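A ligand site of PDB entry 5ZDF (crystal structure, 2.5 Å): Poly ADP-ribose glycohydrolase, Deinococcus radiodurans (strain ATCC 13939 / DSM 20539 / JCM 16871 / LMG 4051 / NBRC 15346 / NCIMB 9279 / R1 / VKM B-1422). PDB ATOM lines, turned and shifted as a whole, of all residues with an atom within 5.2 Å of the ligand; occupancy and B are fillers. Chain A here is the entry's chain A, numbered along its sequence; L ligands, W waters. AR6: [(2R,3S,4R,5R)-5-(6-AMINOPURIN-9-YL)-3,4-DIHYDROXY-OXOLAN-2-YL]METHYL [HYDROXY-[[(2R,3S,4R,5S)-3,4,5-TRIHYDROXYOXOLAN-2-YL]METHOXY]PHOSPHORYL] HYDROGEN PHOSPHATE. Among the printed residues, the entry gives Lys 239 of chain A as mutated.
CA of Thr 45 touches N1 of the ligand, at 3.5 Å. Phe 65 touches the ligand. Ala 66 touches the ligand (C to C3D, 3.8 Å). CB of Ser 67 touches O3D of the ligand, at 3.4 Å. CA of Gly 73 touches O2D of the ligand, at 3.3 Å. Gln 80 touches the ligand (O to N7, 3.7 Å). Ala 81 touches the ligand (CA to O2A, 3.1 Å). O of Ala 194 touches C5' of the ligand, 3.3 Å away. Ala 229 touches the ligand (O to C2, 3.5 Å). Lys 239 touches the ligand. Hydrophobic or aromatic side chains within 4 Å of the ligand: Phe 65, Ala 81, Ala 194, Val 199, Phe 200 and Leu 231. Of the 29 residues printed, 21 come within 4 Å of the ligand.
NE2 of Gln 82 lies within hydrogen-bond range of OG1 of Thr 46. OE1 of Gln 82 sits at hydrogen-bond distance from N of Phe 65 (2.8 Å). The backbone NH (N) of Arg 201 lies within hydrogen-bond range of the backbone carbonyl oxygen (O) of Gly 196. The backbone NH (N) of Ser 67 is in hydrogen-bond range of the side-chain carboxylate (OE1) of Glu 83 (2.7 Å). OE2 of Glu 83 is in hydrogen-bond range of N of Gly 72. O of Ala 194 lies close to SG of Cys 197 (3.5 Å). SG of Cys 197 is in hydrogen-bond range of O of Trp 195, 3.5 Å away. The side-chain carboxylate (OD1) of Asp 232 is in salt-bridge range of the side-chain amino group (NZ) of Lys 239 (3.1 Å).
Water W2 lies within hydrogen-bond range of the backbone carbonyl oxygen (O) of Ala 229 (2.7 Å), a nitrogen (N3) of the ligand (2.9 Å) and the backbone NH (N) of Ala 194 (2.9 Å). Water W1 lies within hydrogen-bond range of O of Ala 66, N of Ala 150, O2B of the ligand and O of Phe 65.
The backbone NH (N) of Leu 231 is in hydrogen-bond range of a nitrogen (N3) of the ligand (3.4 Å). An oxygen (O2') of the ligand sits at hydrogen-bond distance from the backbone carbonyl oxygen (O) of Leu 231, 2.4 Å away. An oxygen (O1B) of the ligand sits at hydrogen-bond distance from the backbone NH of Gly 198 (2.6 Å). An oxygen (O1A) of the ligand is in hydrogen-bond range of the backbone NH of Val 199 (2.7 Å). OD1 of Asp 85 is in hydrogen-bond range of N6 of the ligand, 2.8 Å away. N of Gln 82 sits at hydrogen-bond distance from O2A of the ligand, at 2.8 Å. An oxygen (O2B) of the ligand lies within hydrogen-bond range of the backbone NH (N) of Gly 196, 2.8 Å away. The side-chain carboxylate (OE1) of Glu 83 is in hydrogen-bond range of an oxygen (O2D) of the ligand (2.9 Å). A nitrogen (N1) of the ligand lies within hydrogen-bond range of the backbone NH (N) of Thr 46, 3.0 Å away. The side-chain hydroxyl of Thr 46 lies close to a nitrogen (N1) of the ligand (3.4 Å). An oxygen (O1D) of the ligand is in hydrogen-bond range of the side-chain carboxylate (OE1) of Glu 84, 3.2 Å away. N of Cys 197 lies within hydrogen-bond range of O1B of the ligand. N of Phe 200 is in hydrogen-bond range of O1B of the ligand, 3.4 Å away.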
ATOM      1  N   GLU A  44     -21.491   1.174   9.068  1.00  0.00           N
ATOM      2  CA  GLU A  44     -21.644   2.313   8.182  1.00  0.00           C
ATOM      3  C   GLU A  44     -21.842   3.590   8.989  1.00  0.00           C
ATOM      4  O   GLU A  44     -22.124   3.569  10.198  1.00  0.00           O
ATOM      5  CB  GLU A  44     -22.825   2.124   7.244  1.00  0.00           C
ATOM      6  CG  GLU A  44     -23.895   1.308   7.881  1.00  0.00           C
ATOM      7  CD  GLU A  44     -24.880   0.716   6.909  1.00  0.00           C
ATOM      8  OE1 GLU A  44     -24.811   1.033   5.704  1.00  0.00           O
ATOM      9  OE2 GLU A  44     -25.701  -0.114   7.362  1.00  0.00           O
ATOM     10  N   THR A  45     -21.677   4.716   8.311  1.00  0.00           N
ATOM     11  CA  THR A  45     -22.048   5.953   8.953  1.00  0.00           C
ATOM     12  C   THR A  45     -23.564   6.030   9.075  1.00  0.00           C
ATOM     13  O   THR A  45     -24.306   5.259   8.462  1.00  0.00           O
ATOM     14  CB  THR A  45     -21.540   7.163   8.183  1.00  0.00           C
ATOM     15  OG1 THR A  45     -22.136   7.180   6.884  1.00  0.00           O
ATOM     16  CG2 THR A  45     -20.043   7.117   8.068  1.00  0.00           C
ATOM     17  N   THR A  46     -24.004   6.990   9.869  1.00  0.00           N
ATOM     18  CA  THR A  46     -25.418   7.145  10.138  1.00  0.00           C
ATOM     19  C   THR A  46     -26.172   7.535   8.873  1.00  0.00           C
ATOM     20  O   THR A  46     -27.293   7.057   8.635  1.00  0.00           O
ATOM     21  CB  THR A  46     -25.570   8.159  11.284  1.00  0.00           C
ATOM     22  OG1 THR A  46     -25.199   7.520  12.521  1.00  0.00           O
ATOM     23  CG2 THR A  46     -26.987   8.667  11.376  1.00  0.00           C
ATOM     24  N   PHE A  65     -26.475  12.346  17.584  1.00  0.00           N
ATOM     25  CA  PHE A  65     -25.724  12.290  18.839  1.00  0.00           C
ATOM     26  C   PHE A  65     -25.339  13.728  19.202  1.00  0.00           C
ATOM     27  O   PHE A  65     -24.169  14.136  19.119  1.00  0.00           O
ATOM     28  CB  PHE A  65     -24.491  11.410  18.717  1.00  0.00           C
ATOM     29  CG  PHE A  65     -24.735  10.046  18.096  1.00  0.00           C
ATOM     30  CD1 PHE A  65     -23.659   9.310  17.588  1.00  0.00           C
ATOM     31  CD2 PHE A  65     -26.006   9.482  18.048  1.00  0.00           C
ATOM     32  CE1 PHE A  65     -23.861   8.070  17.032  1.00  0.00           C
ATOM     33  CE2 PHE A  65     -26.199   8.251  17.488  1.00  0.00           C
ATOM     34  CZ  PHE A  65     -25.122   7.534  16.977  1.00  0.00           C
ATOM     35  N   ALA A  66     -26.341  14.485  19.656  1.00  0.00           N
ATOM     36  CA  ALA A  66     -26.265  15.937  19.647  1.00  0.00           C
ATOM     37  C   ALA A  66     -25.524  16.521  20.847  1.00  0.00           C
ATOM     38  O   ALA A  66     -25.426  15.902  21.911  1.00  0.00           O
ATOM     39  CB  ALA A  66     -27.676  16.543  19.607  1.00  0.00           C
ATOM     40  N   SER A  67     -24.994  17.724  20.650  1.00  0.00           N
ATOM     41  CA  SER A  67     -24.661  18.587  21.760  1.00  0.00           C
ATOM     42  C   SER A  67     -25.933  19.091  22.439  1.00  0.00           C
ATOM     43  O   SER A  67     -26.966  19.321  21.794  1.00  0.00           O
ATOM     44  CB  SER A  67     -23.832  19.790  21.289  1.00  0.00           C
ATOM     45  OG  SER A  67     -23.677  20.742  22.324  1.00  0.00           O
ATOM     46  N   GLY A  72     -25.043  21.688  16.323  1.00  0.00           N
ATOM     47  CA  GLY A  72     -23.808  21.221  15.735  1.00  0.00           C
ATOM     48  C   GLY A  72     -22.650  21.152  16.703  1.00  0.00           C
ATOM     49  O   GLY A  72     -21.512  20.866  16.269  1.00  0.00           O
ATOM     50  N   GLY A  73     -22.875  21.418  17.986  1.00  0.00           N
ATOM     51  CA  GLY A  73     -21.791  21.304  18.931  1.00  0.00           C
ATOM     52  C   GLY A  73     -20.622  22.208  18.664  1.00  0.00           C
ATOM     53  O   GLY A  73     -19.533  21.957  19.194  1.00  0.00           O
ATOM     54  N   GLN A  80     -14.267  14.382  14.112  1.00  0.00           N
ATOM     55  CA  GLN A  80     -14.487  13.037  14.644  1.00  0.00           C
ATOM     56  C   GLN A  80     -15.979  12.755  14.859  1.00  0.00           C
ATOM     57  O   GLN A  80     -16.438  11.619  14.645  1.00  0.00           O
ATOM     58  CB  GLN A  80     -13.720  12.881  15.966  1.00  0.00           C
ATOM     59  CG  GLN A  80     -13.819  11.504  16.661  1.00  0.00           C
ATOM     60  CD  GLN A  80     -12.910  11.402  17.894  1.00  0.00           C
ATOM     61  OE1 GLN A  80     -13.031  12.188  18.852  1.00  0.00           O
ATOM     62  NE2 GLN A  80     -11.980  10.429  17.869  1.00  0.00           N
ATOM     63  N   ALA A  81     -16.740  13.774  15.253  1.00  0.00           N
ATOM     64  CA  ALA A  81     -18.052  13.572  15.851  1.00  0.00           C
ATOM     65  C   ALA A  81     -19.153  13.427  14.822  1.00  0.00           C
ATOM     66  O   ALA A  81     -19.121  14.023  13.746  1.00  0.00           O
ATOM     67  CB  ALA A  81     -18.370  14.747  16.764  1.00  0.00           C
ATOM     68  N   GLN A  82     -20.165  12.643  15.190  1.00  0.00           N
ATOM     69  CA  GLN A  82     -21.228  12.283  14.267  1.00  0.00           C
ATOM     70  C   GLN A  82     -22.134  13.469  13.953  1.00  0.00           C
ATOM     71  O   GLN A  82     -22.577  13.635  12.802  1.00  0.00           O
ATOM     72  CB  GLN A  82     -22.035  11.116  14.822  1.00  0.00           C
ATOM     73  CG  GLN A  82     -23.230  10.730  13.972  1.00  0.00           C
ATOM     74  CD  GLN A  82     -24.546  11.005  14.678  1.00  0.00           C
ATOM     75  OE1 GLN A  82     -24.669  11.996  15.424  1.00  0.00           O
ATOM     76  NE2 GLN A  82     -25.542  10.127  14.476  1.00  0.00           N
ATOM     77  N   GLU A  83     -22.453  14.311  14.937  1.00  0.00           N
ATOM     78  CA  GLU A  83     -23.317  15.449  14.647  1.00  0.00           C
ATOM     79  C   GLU A  83     -22.636  16.431  13.691  1.00  0.00           C
ATOM     80  O   GLU A  83     -23.284  17.027  12.826  1.00  0.00           O
ATOM     81  CB  GLU A  83     -23.732  16.174  15.931  1.00  0.00           C
ATOM     82  CG  GLU A  83     -24.311  17.594  15.685  1.00  0.00           C
ATOM     83  CD  GLU A  83     -24.999  18.235  16.898  1.00  0.00           C
ATOM     84  OE1 GLU A  83     -24.446  18.165  18.018  1.00  0.00           O
ATOM     85  OE2 GLU A  83     -26.062  18.869  16.736  1.00  0.00           O
ATOM     86  N   GLU A  84     -21.324  16.605  13.827  1.00  0.00           N
ATOM     87  CA  GLU A  84     -20.571  17.368  12.841  1.00  0.00           C
ATOM     88  C   GLU A  84     -20.732  16.767  11.444  1.00  0.00           C
ATOM     89  O   GLU A  84     -20.957  17.493  10.470  1.00  0.00           O
ATOM     90  CB  GLU A  84     -19.078  17.437  13.238  1.00  0.00           C
ATOM     91  CG  GLU A  84     -18.708  18.427  14.372  1.00  0.00           C
ATOM     92  CD  GLU A  84     -19.295  18.097  15.780  1.00  0.00           C
ATOM     93  OE1 GLU A  84     -18.922  18.814  16.758  1.00  0.00           O
ATOM     94  OE2 GLU A  84     -20.109  17.148  15.916  1.00  0.00           O
ATOM     95  N   ASP A  85     -20.607  15.436  11.344  1.00  0.00           N
ATOM     96  CA  ASP A  85     -20.855  14.757  10.076  1.00  0.00           C
ATOM     97  C   ASP A  85     -22.236  15.097   9.527  1.00  0.00           C
ATOM     98  O   ASP A  85     -22.373  15.463   8.361  1.00  0.00           O
ATOM     99  CB  ASP A  85     -20.719  13.246  10.263  1.00  0.00           C
ATOM    100  CG  ASP A  85     -19.283  12.821  10.461  1.00  0.00           C
ATOM    101  OD1 ASP A  85     -19.055  11.739  11.049  1.00  0.00           O
ATOM    102  OD2 ASP A  85     -18.390  13.573  10.032  1.00  0.00           O
ATOM    103  N   LEU A  86     -23.274  14.967  10.353  1.00  0.00           N
ATOM    104  CA  LEU A  86     -24.626  15.178   9.824  1.00  0.00           C
ATOM    105  C   LEU A  86     -24.834  16.616   9.404  1.00  0.00           C
ATOM    106  O   LEU A  86     -25.497  16.892   8.404  1.00  0.00           O
ATOM    107  CB  LEU A  86     -25.677  14.768  10.846  1.00  0.00           C
ATOM    108  CG  LEU A  86     -25.449  13.491  11.645  1.00  0.00           C
ATOM    109  CD1 LEU A  86     -26.541  13.329  12.688  1.00  0.00           C
ATOM    110  CD2 LEU A  86     -25.378  12.318  10.682  1.00  0.00           C
ATOM    111  N   ALA A 150     -27.120  12.512  24.690  1.00  0.00           N
ATOM    112  CA  ALA A 150     -26.790  11.566  25.743  1.00  0.00           C
ATOM    113  C   ALA A 150     -26.189  12.319  26.920  1.00  0.00           C
ATOM    114  O   ALA A 150     -25.588  13.394  26.747  1.00  0.00           O
ATOM    115  CB  ALA A 150     -25.833  10.503  25.228  1.00  0.00           C
ATOM    116  N   ALA A 194     -23.963   4.342  18.271  1.00  0.00           N
ATOM    117  CA  ALA A 194     -23.181   4.403  19.500  1.00  0.00           C
ATOM    118  C   ALA A 194     -23.427   5.720  20.245  1.00  0.00           C
ATOM    119  O   ALA A 194     -22.505   6.491  20.526  1.00  0.00           O
ATOM    120  CB  ALA A 194     -21.703   4.210  19.189  1.00  0.00           C
ATOM    121  N   TRP A 195     -24.710   5.946  20.576  1.00  0.00           N
ATOM    122  CA  TRP A 195     -25.164   7.192  21.206  1.00  0.00           C
ATOM    123  C   TRP A 195     -24.417   7.450  22.517  1.00  0.00           C
ATOM    124  O   TRP A 195     -24.481   6.658  23.460  1.00  0.00           O
ATOM    125  CB  TRP A 195     -26.674   7.094  21.483  1.00  0.00           C
ATOM    126  CG  TRP A 195     -27.306   8.379  21.884  1.00  0.00           C
ATOM    127  CD1 TRP A 195     -27.027   9.605  21.366  1.00  0.00           C
ATOM    128  CD2 TRP A 195     -28.325   8.585  22.881  1.00  0.00           C
ATOM    129  NE1 TRP A 195     -27.804  10.561  21.969  1.00  0.00           N
ATOM    130  CE2 TRP A 195     -28.610   9.962  22.902  1.00  0.00           C
ATOM    131  CE3 TRP A 195     -29.022   7.751  23.760  1.00  0.00           C
ATOM    132  CZ2 TRP A 195     -29.566  10.529  23.763  1.00  0.00           C
ATOM    133  CZ3 TRP A 195     -29.978   8.309  24.623  1.00  0.00           C
ATOM    134  CH2 TRP A 195     -30.237   9.689  24.609  1.00  0.00           C
ATOM    135  N   GLY A 196     -23.706   8.578  22.577  1.00  0.00           N
ATOM    136  CA  GLY A 196     -23.037   8.973  23.801  1.00  0.00           C
ATOM    137  C   GLY A 196     -21.677   8.366  24.001  1.00  0.00           C
ATOM    138  O   GLY A 196     -20.983   8.751  24.947  1.00  0.00           O
ATOM    139  N   CYS A 197     -21.265   7.443  23.132  1.00  0.00           N
ATOM    140  CA  CYS A 197     -20.125   6.584  23.397  1.00  0.00           C
ATOM    141  C   CYS A 197     -18.787   7.166  22.931  1.00  0.00           C
ATOM    142  O   CYS A 197     -17.753   6.549  23.186  1.00  0.00           O
ATOM    143  CB  CYS A 197     -20.343   5.214  22.743  1.00  0.00           C
ATOM    144  SG  CYS A 197     -21.871   4.389  23.268  1.00  0.00           S
ATOM    145  N   GLY A 198     -18.782   8.314  22.259  1.00  0.00           N
ATOM    146  CA  GLY A 198     -17.533   8.879  21.808  1.00  0.00           C
ATOM    147  C   GLY A 198     -17.052  10.042  22.670  1.00  0.00           C
ATOM    148  O   GLY A 198     -16.461   9.828  23.729  1.00  0.00           O
ATOM    149  N   VAL A 199     -17.322  11.259  22.206  1.00  0.00           N
ATOM    150  CA  VAL A 199     -16.936  12.460  22.940  1.00  0.00           C
ATOM    151  C   VAL A 199     -17.442  12.400  24.380  1.00  0.00           C
ATOM    152  O   VAL A 199     -16.701  12.743  25.318  1.00  0.00           O
ATOM    153  CB  VAL A 199     -17.480  13.710  22.209  1.00  0.00           C
ATOM    154  CG1 VAL A 199     -17.168  14.981  22.991  1.00  0.00           C
ATOM    155  CG2 VAL A 199     -16.918  13.787  20.809  1.00  0.00           C
ATOM    156  N   PHE A 200     -18.688  11.943  24.586  1.00  0.00           N
ATOM    157  CA  PHE A 200     -19.351  11.940  25.892  1.00  0.00           C
ATOM    158  C   PHE A 200     -18.958  10.759  26.775  1.00  0.00           C
ATOM    159  O   PHE A 200     -19.312  10.775  27.966  1.00  0.00           O
ATOM    160  CB  PHE A 200     -20.875  11.953  25.720  1.00  0.00           C
ATOM    161  CG  PHE A 200     -21.440  13.305  25.433  1.00  0.00           C
ATOM    162  CD1 PHE A 200     -20.606  14.406  25.349  1.00  0.00           C
ATOM    163  CD2 PHE A 200     -22.801  13.496  25.238  1.00  0.00           C
ATOM    164  CE1 PHE A 200     -21.112  15.669  25.081  1.00  0.00           C
ATOM    165  CE2 PHE A 200     -23.319  14.757  24.952  1.00  0.00           C
ATOM    166  CZ  PHE A 200     -22.474  15.839  24.879  1.00  0.00           C
ATOM    167  N   ARG A 201     -18.307   9.741  26.220  1.00  0.00           N
ATOM    168  CA  ARG A 201     -17.542   8.739  26.980  1.00  0.00           C
ATOM    169  C   ARG A 201     -18.431   7.740  27.730  1.00  0.00           C
ATOM    170  O   ARG A 201     -18.006   7.173  28.742  1.00  0.00           O
ATOM    171  CB  ARG A 201     -16.584   9.425  27.960  1.00  0.00           C
ATOM    172  CG  ARG A 201     -15.504  10.178  27.261  1.00  0.00           C
ATOM    173  CD  ARG A 201     -14.307   9.329  27.250  1.00  0.00           C
ATOM    174  NE  ARG A 201     -13.698   9.230  25.938  1.00  0.00           N
ATOM    175  CZ  ARG A 201     -12.638   9.932  25.569  1.00  0.00           C
ATOM    176  NH1 ARG A 201     -12.072  10.773  26.448  1.00  0.00           N
ATOM    177  NH2 ARG A 201     -12.119   9.778  24.350  1.00  0.00           N
ATOM    178  N   ALA A 229     -25.984   1.923  12.869  1.00  0.00           N
ATOM    179  CA  ALA A 229     -24.815   2.273  12.078  1.00  0.00           C
ATOM    180  C   ALA A 229     -23.725   2.779  13.022  1.00  0.00           C
ATOM    181  O   ALA A 229     -23.822   3.893  13.548  1.00  0.00           O
ATOM    182  CB  ALA A 229     -25.203   3.312  11.026  1.00  0.00           C
ATOM    183  N   VAL A 230     -22.680   1.972  13.238  1.00  0.00           N
ATOM    184  CA  VAL A 230     -21.623   2.308  14.197  1.00  0.00           C
ATOM    185  C   VAL A 230     -20.303   2.452  13.445  1.00  0.00           C
ATOM    186  O   VAL A 230     -19.615   1.447  13.191  1.00  0.00           O
ATOM    187  CB  VAL A 230     -21.499   1.272  15.314  1.00  0.00           C
ATOM    188  CG1 VAL A 230     -20.355   1.653  16.243  1.00  0.00           C
ATOM    189  CG2 VAL A 230     -22.799   1.160  16.068  1.00  0.00           C
ATOM    190  N   LEU A 231     -19.920   3.680  13.109  1.00  0.00           N
ATOM    191  CA  LEU A 231     -18.579   3.916  12.583  1.00  0.00           C
ATOM    192  C   LEU A 231     -17.556   3.560  13.653  1.00  0.00           C
ATOM    193  O   LEU A 231     -17.752   3.850  14.845  1.00  0.00           O
ATOM    194  CB  LEU A 231     -18.437   5.368  12.135  1.00  0.00           C
ATOM    195  CG  LEU A 231     -17.224   5.777  11.277  1.00  0.00           C
ATOM    196  CD1 LEU A 231     -17.216   4.989   9.975  1.00  0.00           C
ATOM    197  CD2 LEU A 231     -17.210   7.272  11.001  1.00  0.00           C
ATOM    198  N   ASP A 232     -16.474   2.895  13.254  1.00  0.00           N
ATOM    199  CA  ASP A 232     -15.467   2.439  14.221  1.00  0.00           C
ATOM    200  C   ASP A 232     -14.180   2.122  13.455  1.00  0.00           C
ATOM    201  O   ASP A 232     -13.974   0.991  13.000  1.00  0.00           O
ATOM    202  CB  ASP A 232     -15.955   1.230  14.998  1.00  0.00           C
ATOM    203  CG  ASP A 232     -15.274   1.080  16.351  1.00  0.00           C
ATOM    204  OD1 ASP A 232     -14.131   1.566  16.523  1.00  0.00           O
ATOM    205  OD2 ASP A 232     -15.893   0.464  17.251  1.00  0.00           O
ATOM    206  N   LYS A 239     -16.273  -0.113  20.195  1.00  0.00           N
ATOM    207  CA  LYS A 239     -17.688   0.268  20.094  1.00  0.00           C
ATOM    208  C   LYS A 239     -18.441  -0.698  19.191  1.00  0.00           C
ATOM    209  O   LYS A 239     -19.455  -1.285  19.584  1.00  0.00           O
ATOM    210  CB  LYS A 239     -17.796   1.709  19.578  1.00  0.00           C
ATOM    211  CG  LYS A 239     -17.304   2.781  20.548  1.00  0.00           C
ATOM    212  CD  LYS A 239     -17.090   4.100  19.817  1.00  0.00           C
ATOM    213  CE  LYS A 239     -15.617   4.416  19.680  1.00  0.00           C
ATOM    214  NZ  LYS A 239     -14.957   3.827  18.471  1.00  0.00           N
HETATM  215  N1  AR6 L   1     -21.909   7.923  11.823  1.00  0.00           N
HETATM  216  C2  AR6 L   1     -22.133   6.877  12.659  1.00  0.00           C
HETATM  217  N3  AR6 L   1     -21.393   6.713  13.771  1.00  0.00           N
HETATM  218  C4  AR6 L   1     -20.430   7.601  14.026  1.00  0.00           C
HETATM  219  C5  AR6 L   1     -20.194   8.640  13.210  1.00  0.00           C
HETATM  220  C6  AR6 L   1     -20.967   8.802  12.082  1.00  0.00           C
HETATM  221  N6  AR6 L   1     -21.006   9.774  11.008  1.00  0.00           N
HETATM  222  N7  AR6 L   1     -19.184   9.361  13.715  1.00  0.00           N
HETATM  223  C8  AR6 L   1     -18.806   8.763  14.841  1.00  0.00           C
HETATM  224  N9  AR6 L   1     -19.564   7.684  15.046  1.00  0.00           N
HETATM  225  PA  AR6 L   1     -19.923  11.060  19.035  1.00  0.00           P
HETATM  226  PB  AR6 L   1     -21.302  11.393  21.553  1.00  0.00           P
HETATM  227  C1' AR6 L   1     -19.444   6.771  16.109  1.00  0.00           C
HETATM  228  O1A AR6 L   1     -18.737  11.203  19.941  1.00  0.00           O
HETATM  229  O1B AR6 L   1     -20.360  10.357  22.122  1.00  0.00           O
HETATM  230  C1D AR6 L   1     -20.148  16.125  19.265  1.00  0.00           C
HETATM  231  O1D AR6 L   1     -19.291  17.081  19.388  1.00  0.00           O
HETATM  232  C2' AR6 L   1     -18.170   6.765  16.539  1.00  0.00           C
HETATM  233  O2' AR6 L   1     -17.676   5.387  16.737  1.00  0.00           O
HETATM  234  O2A AR6 L   1     -19.854  11.995  17.871  1.00  0.00           O
HETATM  235  O2B AR6 L   1     -22.726  11.171  21.984  1.00  0.00           O
HETATM  236  C2D AR6 L   1     -21.573  16.606  19.537  1.00  0.00           C
HETATM  237  O2D AR6 L   1     -21.752  18.012  19.108  1.00  0.00           O
HETATM  238  C3' AR6 L   1     -18.172   7.550  17.881  1.00  0.00           C
HETATM  239  O3' AR6 L   1     -17.203   7.139  18.701  1.00  0.00           O
HETATM  240  O3A AR6 L   1     -21.290  11.325  19.903  1.00  0.00           O
HETATM  241  C3D AR6 L   1     -21.701  16.504  20.864  1.00  0.00           C
HETATM  242  O3D AR6 L   1     -21.177  17.667  21.505  1.00  0.00           O
HETATM  243  C4' AR6 L   1     -19.630   7.272  18.451  1.00  0.00           C
HETATM  244  O4' AR6 L   1     -20.391   7.190  17.386  1.00  0.00           O
HETATM  245  C4D AR6 L   1     -20.792  15.209  21.300  1.00  0.00           C
HETATM  246  O4D AR6 L   1     -19.895  15.017  20.378  1.00  0.00           O
HETATM  247  C5' AR6 L   1     -20.119   8.444  19.294  1.00  0.00           C
HETATM  248  O5' AR6 L   1     -20.039   9.546  18.426  1.00  0.00           O
HETATM  249  C5D AR6 L   1     -21.658  13.989  21.401  1.00  0.00           C
HETATM  250  O5D AR6 L   1     -20.888  12.942  21.964  1.00  0.00           O
HETATM  251  O   HOH W   1     -25.358  13.072  22.226  1.00  0.00           O
HETATM  252  O   HOH W   2     -22.843   5.130  15.705  1.00  0.00           O
